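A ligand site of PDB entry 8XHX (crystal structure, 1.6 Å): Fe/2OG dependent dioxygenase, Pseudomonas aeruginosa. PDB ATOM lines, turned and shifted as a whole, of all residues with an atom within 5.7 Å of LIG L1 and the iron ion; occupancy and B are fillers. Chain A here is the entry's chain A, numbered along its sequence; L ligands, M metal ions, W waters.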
ATOM      1  N   GLN A  94      19.691   3.665  34.946  1.00  0.00           N
ATOM      2  CA  GLN A  94      20.732   4.600  34.526  1.00  0.00           C
ATOM      3  C   GLN A  94      22.057   4.275  35.197  1.00  0.00           C
ATOM      4  O   GLN A  94      22.114   3.673  36.265  1.00  0.00           O
ATOM      5  CB  GLN A  94      20.329   6.032  34.874  1.00  0.00           C
ATOM      6  CG  GLN A  94      19.109   6.513  34.101  1.00  0.00           C
ATOM      7  CD  GLN A  94      18.582   7.827  34.643  1.00  0.00           C
ATOM      8  OE1 GLN A  94      18.351   7.957  35.850  1.00  0.00           O
ATOM      9  NE2 GLN A  94      18.415   8.813  33.766  1.00  0.00           N
ATOM     10  N   THR A 156      26.886   9.508  31.209  1.00  0.00           N
ATOM     11  CA  THR A 156      25.674   8.973  31.831  1.00  0.00           C
ATOM     12  C   THR A 156      24.903   8.157  30.813  1.00  0.00           C
ATOM     13  O   THR A 156      24.696   8.616  29.684  1.00  0.00           O
ATOM     14  CB  THR A 156      24.813  10.102  32.388  1.00  0.00           C
ATOM     15  OG1 THR A 156      25.461  10.677  33.523  1.00  0.00           O
ATOM     16  CG2 THR A 156      23.436   9.566  32.813  1.00  0.00           C
ATOM     17  N   ASN A 158      21.497   5.731  29.726  1.00  0.00           N
ATOM     18  CA  ASN A 158      20.074   5.432  29.868  1.00  0.00           C
ATOM     19  C   ASN A 158      19.811   4.094  29.192  1.00  0.00           C
ATOM     20  O   ASN A 158      20.098   3.955  27.996  1.00  0.00           O
ATOM     21  CB  ASN A 158      19.204   6.494  29.195  1.00  0.00           C
ATOM     22  CG  ASN A 158      19.299   7.846  29.855  1.00  0.00           C
ATOM     23  OD1 ASN A 158      19.089   7.968  31.059  1.00  0.00           O
ATOM     24  ND2 ASN A 158      19.602   8.860  29.061  1.00  0.00           N
ATOM     25  N   PHE A 160      16.403   2.034  28.453  1.00  0.00           N
ATOM     26  CA  PHE A 160      14.948   2.164  28.528  1.00  0.00           C
ATOM     27  C   PHE A 160      14.342   0.776  28.657  1.00  0.00           C
ATOM     28  O   PHE A 160      14.288   0.026  27.683  1.00  0.00           O
ATOM     29  CB  PHE A 160      14.411   2.924  27.312  1.00  0.00           C
ATOM     30  CG  PHE A 160      14.845   4.366  27.279  1.00  0.00           C
ATOM     31  CD1 PHE A 160      13.999   5.367  27.740  1.00  0.00           C
ATOM     32  CD2 PHE A 160      16.110   4.712  26.832  1.00  0.00           C
ATOM     33  CE1 PHE A 160      14.420   6.703  27.741  1.00  0.00           C
ATOM     34  CE2 PHE A 160      16.534   6.037  26.819  1.00  0.00           C
ATOM     35  CZ  PHE A 160      15.693   7.030  27.280  1.00  0.00           C
ATOM     36  N   LEU A 169      11.387   8.793  29.647  1.00  0.00           N
ATOM     37  CA  LEU A 169      12.145   9.679  30.520  1.00  0.00           C
ATOM     38  C   LEU A 169      11.335  10.949  30.665  1.00  0.00           C
ATOM     39  O   LEU A 169      10.899  11.520  29.657  1.00  0.00           O
ATOM     40  CB  LEU A 169      13.533   9.971  29.944  1.00  0.00           C
ATOM     41  CG  LEU A 169      14.410  10.962  30.730  1.00  0.00           C
ATOM     42  CD1 LEU A 169      14.615  10.466  32.141  1.00  0.00           C
ATOM     43  CD2 LEU A 169      15.744  11.164  30.036  1.00  0.00           C
ATOM     44  N   HIS A 172      12.237  17.285  31.277  1.00  0.00           N
ATOM     45  CA  HIS A 172      13.296  17.903  32.076  1.00  0.00           C
ATOM     46  C   HIS A 172      14.076  18.894  31.217  1.00  0.00           C
ATOM     47  O   HIS A 172      14.014  18.863  29.985  1.00  0.00           O
ATOM     48  CB  HIS A 172      14.255  16.850  32.644  1.00  0.00           C
ATOM     49  CG  HIS A 172      15.059  16.151  31.581  1.00  0.00           C
ATOM     50  ND1 HIS A 172      14.545  15.134  30.803  1.00  0.00           N
ATOM     51  CD2 HIS A 172      16.332  16.345  31.164  1.00  0.00           C
ATOM     52  CE1 HIS A 172      15.474  14.726  29.954  1.00  0.00           C
ATOM     53  NE2 HIS A 172      16.568  15.443  30.153  1.00  0.00           N
ATOM     54  N   LYS A 173      14.836  19.737  31.899  1.00  0.00           N
ATOM     55  CA  LYS A 173      15.973  20.416  31.294  1.00  0.00           C
ATOM     56  C   LYS A 173      17.232  19.807  31.869  1.00  0.00           C
ATOM     57  O   LYS A 173      17.232  19.377  33.026  1.00  0.00           O
ATOM     58  CB  LYS A 173      15.941  21.921  31.590  1.00  0.00           C
ATOM     59  CG  LYS A 173      14.853  22.680  30.838  1.00  0.00           C
ATOM     60  CD  LYS A 173      14.825  24.159  31.287  1.00  0.00           C
ATOM     61  CE  LYS A 173      13.759  24.957  30.545  1.00  0.00           C
ATOM     62  NZ  LYS A 173      13.737  26.380  31.026  1.00  0.00           N
ATOM     63  N   ASP A 174      18.279  19.704  31.055  1.00  0.00           N
ATOM     64  CA  ASP A 174      19.574  19.303  31.578  1.00  0.00           C
ATOM     65  C   ASP A 174      20.124  20.422  32.468  1.00  0.00           C
ATOM     66  O   ASP A 174      19.769  21.598  32.316  1.00  0.00           O
ATOM     67  CB  ASP A 174      20.567  19.014  30.452  1.00  0.00           C
ATOM     68  CG  ASP A 174      20.178  17.814  29.600  1.00  0.00           C
ATOM     69  OD1 ASP A 174      19.194  17.097  29.902  1.00  0.00           O
ATOM     70  OD2 ASP A 174      20.887  17.575  28.598  1.00  0.00           O
ATOM     71  N   THR A 179      25.359  19.380  26.571  1.00  0.00           N
ATOM     72  CA  THR A 179      25.242  17.929  26.619  1.00  0.00           C
ATOM     73  C   THR A 179      25.503  17.421  25.208  1.00  0.00           C
ATOM     74  O   THR A 179      24.911  17.933  24.249  1.00  0.00           O
ATOM     75  CB  THR A 179      23.835  17.520  27.054  1.00  0.00           C
ATOM     76  OG1 THR A 179      23.569  18.046  28.365  1.00  0.00           O
ATOM     77  CG2 THR A 179      23.682  16.006  27.056  1.00  0.00           C
ATOM     78  N   LEU A 181      25.004  14.195  23.053  1.00  0.00           N
ATOM     79  CA  LEU A 181      24.137  13.028  23.206  1.00  0.00           C
ATOM     80  C   LEU A 181      24.349  12.007  22.084  1.00  0.00           C
ATOM     81  O   LEU A 181      24.257  12.360  20.898  1.00  0.00           O
ATOM     82  CB  LEU A 181      22.667  13.452  23.253  1.00  0.00           C
ATOM     83  CG  LEU A 181      21.579  12.365  23.182  1.00  0.00           C
ATOM     84  CD1 LEU A 181      21.578  11.498  24.467  1.00  0.00           C
ATOM     85  CD2 LEU A 181      20.225  13.057  23.005  1.00  0.00           C
ATOM     86  N   SER A 183      22.785   8.738  20.481  1.00  0.00           N
ATOM     87  CA  SER A 183      21.590   7.919  20.402  1.00  0.00           C
ATOM     88  C   SER A 183      21.418   7.399  18.986  1.00  0.00           C
ATOM     89  O   SER A 183      22.039   7.896  18.045  1.00  0.00           O
ATOM     90  CB  SER A 183      20.336   8.694  20.844  1.00  0.00           C
ATOM     91  OG  SER A 183      20.211   9.910  20.095  1.00  0.00           O
ATOM     92  N   GLY A 187      12.446   8.812  19.742  1.00  0.00           N
ATOM     93  CA  GLY A 187      11.943   8.818  21.099  1.00  0.00           C
ATOM     94  C   GLY A 187      12.091  10.172  21.761  1.00  0.00           C
ATOM     95  O   GLY A 187      11.237  10.593  22.545  1.00  0.00           O
ATOM     96  N   LEU A 188      13.189  10.859  21.468  1.00  0.00           N
ATOM     97  CA  LEU A 188      13.405  12.207  21.990  1.00  0.00           C
ATOM     98  C   LEU A 188      12.398  13.174  21.376  1.00  0.00           C
ATOM     99  O   LEU A 188      12.199  13.181  20.162  1.00  0.00           O
ATOM    100  CB  LEU A 188      14.833  12.674  21.693  1.00  0.00           C
ATOM    101  CG  LEU A 188      15.184  14.122  22.065  1.00  0.00           C
ATOM    102  CD1 LEU A 188      15.187  14.282  23.589  1.00  0.00           C
ATOM    103  CD2 LEU A 188      16.544  14.492  21.486  1.00  0.00           C
ATOM    104  N   ASN A 209      22.715  19.846  23.241  1.00  0.00           N
ATOM    105  CA  ASN A 209      21.723  20.772  23.775  1.00  0.00           C
ATOM    106  C   ASN A 209      22.305  21.558  24.926  1.00  0.00           C
ATOM    107  O   ASN A 209      23.326  21.187  25.517  1.00  0.00           O
ATOM    108  CB  ASN A 209      20.420  20.055  24.183  1.00  0.00           C
ATOM    109  CG  ASN A 209      20.605  19.106  25.337  1.00  0.00           C
ATOM    110  OD1 ASN A 209      20.848  17.911  25.141  1.00  0.00           O
ATOM    111  ND2 ASN A 209      20.433  19.608  26.549  1.00  0.00           N
ATOM    112  N   HIS A 230      12.713  18.713  27.411  1.00  0.00           N
ATOM    113  CA  HIS A 230      12.672  17.595  26.489  1.00  0.00           C
ATOM    114  C   HIS A 230      12.324  16.342  27.277  1.00  0.00           C
ATOM    115  O   HIS A 230      12.396  16.320  28.511  1.00  0.00           O
ATOM    116  CB  HIS A 230      13.991  17.440  25.703  1.00  0.00           C
ATOM    117  CG  HIS A 230      15.218  17.396  26.554  1.00  0.00           C
ATOM    118  ND1 HIS A 230      15.741  18.522  27.174  1.00  0.00           N
ATOM    119  CD2 HIS A 230      16.067  16.377  26.845  1.00  0.00           C
ATOM    120  CE1 HIS A 230      16.829  18.177  27.846  1.00  0.00           C
ATOM    121  NE2 HIS A 230      17.053  16.895  27.652  1.00  0.00           N
ATOM    122  N   ARG A 231      11.957  15.284  26.554  1.00  0.00           N
ATOM    123  CA  ARG A 231      11.447  14.057  27.153  1.00  0.00           C
ATOM    124  C   ARG A 231      11.716  12.911  26.192  1.00  0.00           C
ATOM    125  O   ARG A 231      12.077  13.131  25.036  1.00  0.00           O
ATOM    126  CB  ARG A 231       9.941  14.159  27.446  1.00  0.00           C
ATOM    127  CG  ARG A 231       9.106  14.255  26.186  1.00  0.00           C
ATOM    128  CD  ARG A 231       7.623  14.519  26.455  1.00  0.00           C
ATOM    129  NE  ARG A 231       6.863  14.339  25.221  1.00  0.00           N
ATOM    130  CZ  ARG A 231       5.583  14.668  25.079  1.00  0.00           C
ATOM    131  NH1 ARG A 231       4.928  15.202  26.096  1.00  0.00           N
ATOM    132  NH2 ARG A 231       4.969  14.471  23.917  1.00  0.00           N
ATOM    133  N   VAL A 232      11.545  11.672  26.668  1.00  0.00           N
ATOM    134  CA  VAL A 232      11.595  10.499  25.817  1.00  0.00           C
ATOM    135  C   VAL A 232      10.286   9.729  25.948  1.00  0.00           C
ATOM    136  O   VAL A 232       9.865   9.392  27.067  1.00  0.00           O
ATOM    137  CB  VAL A 232      12.801   9.586  26.127  1.00  0.00           C
ATOM    138  CG1 VAL A 232      12.811   8.380  25.181  1.00  0.00           C
ATOM    139  CG2 VAL A 232      14.110  10.365  25.964  1.00  0.00           C
ATOM    140  N   ARG A 242      15.778   0.485  23.643  1.00  0.00           N
ATOM    141  CA  ARG A 242      16.436   1.743  23.344  1.00  0.00           C
ATOM    142  C   ARG A 242      17.474   2.039  24.406  1.00  0.00           C
ATOM    143  O   ARG A 242      17.276   1.727  25.587  1.00  0.00           O
ATOM    144  CB  ARG A 242      15.400   2.873  23.304  1.00  0.00           C
ATOM    145  CG  ARG A 242      15.941   4.187  22.776  1.00  0.00           C
ATOM    146  CD  ARG A 242      14.825   5.222  22.731  1.00  0.00           C
ATOM    147  NE  ARG A 242      15.260   6.456  22.067  1.00  0.00           N
ATOM    148  CZ  ARG A 242      15.940   7.423  22.668  1.00  0.00           C
ATOM    149  NH1 ARG A 242      16.270   7.328  23.951  1.00  0.00           N
ATOM    150  NH2 ARG A 242      16.285   8.507  21.967  1.00  0.00           N
ATOM    151  N   PHE A 243      18.593   2.638  23.986  1.00  0.00           N
ATOM    152  CA  PHE A 243      19.551   3.215  24.920  1.00  0.00           C
ATOM    153  C   PHE A 243      19.977   4.584  24.424  1.00  0.00           C
ATOM    154  O   PHE A 243      19.816   4.925  23.249  1.00  0.00           O
ATOM    155  CB  PHE A 243      20.808   2.334  25.138  1.00  0.00           C
ATOM    156  CG  PHE A 243      21.693   2.186  23.912  1.00  0.00           C
ATOM    157  CD1 PHE A 243      22.640   3.158  23.595  1.00  0.00           C
ATOM    158  CD2 PHE A 243      21.607   1.066  23.104  1.00  0.00           C
ATOM    159  CE1 PHE A 243      23.465   3.021  22.492  1.00  0.00           C
ATOM    160  CE2 PHE A 243      22.432   0.929  22.001  1.00  0.00           C
ATOM    161  CZ  PHE A 243      23.363   1.915  21.693  1.00  0.00           C
ATOM    162  N   SER A 244      20.540   5.372  25.342  1.00  0.00           N
ATOM    163  CA  SER A 244      21.239   6.581  24.946  1.00  0.00           C
ATOM    164  C   SER A 244      22.303   6.834  25.997  1.00  0.00           C
ATOM    165  O   SER A 244      22.242   6.297  27.110  1.00  0.00           O
ATOM    166  CB  SER A 244      20.300   7.787  24.823  1.00  0.00           C
ATOM    167  OG  SER A 244      19.639   8.044  26.055  1.00  0.00           O
ATOM    168  N   ALA A 246      25.316  10.163  27.190  1.00  0.00           N
ATOM    169  CA  ALA A 246      25.711  11.516  26.845  1.00  0.00           C
ATOM    170  C   ALA A 246      26.821  11.979  27.760  1.00  0.00           C
ATOM    171  O   ALA A 246      26.968  11.503  28.891  1.00  0.00           O
ATOM    172  CB  ALA A 246      24.515  12.489  26.928  1.00  0.00           C
ATOM    173  N   PHE A 248      27.707  15.056  29.787  1.00  0.00           N
ATOM    174  CA  PHE A 248      27.122  16.258  30.374  1.00  0.00           C
ATOM    175  C   PHE A 248      28.232  17.112  30.955  1.00  0.00           C
ATOM    176  O   PHE A 248      28.997  16.631  31.785  1.00  0.00           O
ATOM    177  CB  PHE A 248      26.125  15.908  31.493  1.00  0.00           C
ATOM    178  CG  PHE A 248      24.909  15.156  31.027  1.00  0.00           C
ATOM    179  CD1 PHE A 248      23.723  15.829  30.784  1.00  0.00           C
ATOM    180  CD2 PHE A 248      24.950  13.783  30.850  1.00  0.00           C
ATOM    181  CE1 PHE A 248      22.589  15.136  30.360  1.00  0.00           C
ATOM    182  CE2 PHE A 248      23.826  13.085  30.417  1.00  0.00           C
ATOM    183  CZ  PHE A 248      22.641  13.771  30.179  1.00  0.00           C
HETATM  184  C1  LIG L   1      19.123  12.818  29.095  1.00  0.00           C
HETATM  185  O1  LIG L   1      19.710  11.765  29.441  1.00  0.00           O
HETATM  186  O2  LIG L   1      19.228  13.884  29.738  1.00  0.00           O
HETATM  187  C2  LIG L   1      18.290  12.809  27.909  1.00  0.00           C
HETATM  188  O3  LIG L   1      17.647  13.814  27.660  1.00  0.00           O
HETATM  189  C3  LIG L   1      18.239  11.564  27.037  1.00  0.00           C
HETATM  190  C4  LIG L   1      17.530  11.794  25.690  1.00  0.00           C
HETATM  191  C5  LIG L   1      17.466  10.552  24.814  1.00  0.00           C
HETATM  192  O4  LIG L   1      17.303  10.719  23.579  1.00  0.00           O
HETATM  193  O5  LIG L   1      17.530   9.420  25.345  1.00  0.00           O
HETATM  194  C1  LG2 L   2      24.155  15.522  34.809  1.00  0.00           C
HETATM  195  C2  LG2 L   2      23.815  14.193  34.157  1.00  0.00           C
HETATM  196  C3  LG2 L   2      21.401  14.918  33.574  1.00  0.00           C
HETATM  197  C4  LG2 L   2      21.839  16.319  33.972  1.00  0.00           C
HETATM  198  C5  LG2 L   2      20.343  14.433  34.572  1.00  0.00           C
HETATM  199  C6  LG2 L   2      24.425  15.320  36.307  1.00  0.00           C
HETATM  200  C7  LG2 L   2      19.172  13.659  33.951  1.00  0.00           C
HETATM  201  C8  LG2 L   2      19.648  12.399  33.232  1.00  0.00           C
HETATM  202  C9  LG2 L   2      18.370  14.524  32.984  1.00  0.00           C
HETATM  203  C10 LG2 L   2      24.935  16.644  36.896  1.00  0.00           C
HETATM  204  C11 LG2 L   2      23.170  14.844  37.016  1.00  0.00           C
HETATM  205  C12 LG2 L   2      23.397  14.586  38.514  1.00  0.00           C
HETATM  206  N1  LG2 L   2      23.165  16.578  34.566  1.00  0.00           N
HETATM  207  N2  LG2 L   2      22.514  13.951  33.568  1.00  0.00           N
HETATM  208  O1  LG2 L   2      21.078  17.219  33.766  1.00  0.00           O
HETATM  209  O2  LG2 L   2      24.661  13.342  34.110  1.00  0.00           O
HETATM  210  O3  LG2 L   2      18.328  13.265  34.991  1.00  0.00           O
HETATM  211  O4  LG2 L   2      24.389  13.629  38.728  1.00  0.00           O
HETATM  212 FE    FE M   1      18.260  15.480  28.852  1.00  0.00          FE
HETATM  213  O   HOH W   1      19.003  15.466  24.902  1.00  0.00           O
HETATM  214  O   HOH W   2      17.897  11.076  20.827  1.00  0.00           O
HETATM  215  O   HOH W   3      19.912  15.531  27.379  1.00  0.00           O
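Three residues have an atom within 4 Å of the iron ion: His 172, Asp 174 and His 230.
ND2 of Asn 158 sits at hydrogen-bond distance from O1 of LIG L1 (2.9 Å).
O5 of LIG L1 lies within salt-bridge range of NH1 of Arg 242 (2.8 Å).
An oxygen (O2) of LG2 L2 sits at hydrogen-bond distance from the side-chain hydroxyl (OG1) of Thr 156 (2.8 Å).
OG of Ser 244 lies within hydrogen-bond range of O5 of LIG L1.
Water W3 lies within hydrogen-bond range of OD2 of Asp 174 (2.6 Å) and OD1 of Asn 209 (3.4 Å).
Water W2 lies within hydrogen-bond range of OG of Ser 183, O4 of LIG L1 and NH2 of Arg 242.
The side-chain carboxylate (OD2) of Asp 174 sits at hydrogen-bond distance from the side-chain amide nitrogen (ND2) of Asn 209 (2.9 Å).
The backbone NH (N) of Phe 160 is in hydrogen-bond range of the backbone carbonyl oxygen (O) of Arg 242.
The side-chain carboxylate (OD2) of Asp 174 sits at hydrogen-bond distance from the side-chain hydroxyl (OG1) of Thr 179 (2.7 Å).
The side-chain amide oxygen (OD1) of Asn 158 sits at hydrogen-bond distance from the side-chain amide nitrogen (NE2) of Gln 94 (2.9 Å).
The backbone NH (N) of Leu 169 sits at hydrogen-bond distance from the backbone carbonyl oxygen (O) of Val 232 (3.1 Å).
O of Ser 244 is in hydrogen-bond range of N of Asn 158 (2.8 Å).
The iron ion is bound by an oxygen (O2) of LIG L1 (2.1 Å), a ring nitrogen (NE2) of His 172 (2.1 Å), an oxygen (O3) of LIG L1 (2.1 Å), the side-chain carboxylate (OD1) of Asp 174 (2.1 Å), a ring nitrogen (NE2) of His 230 (2.2 Å) and water W3 (2.2 Å).
Phe 160 touches LIG L1.
CD2 of Leu 169 touches C2 of LIG L1, 3.7 Å away.
Leu 181 touches LIG L1.
CB of Leu 188 touches O4 of LIG L1 (3.7 Å).
Val 232 touches LIG L1 (CG2 to C5, 3.6 Å).
Phe 248 touches LIG L1.
Hydrophobic or aromatic side chains that line LIG L1: Phe 160, Leu 169, His 172, Leu 181, Leu 188, His 230, Val 232 and Phe 248.
Of the 22 residues printed, 12 come within 4 Å of LIG L1.
The nearest printed residue that does not touch LIG L1 is Ser 183 (4.6 Å).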
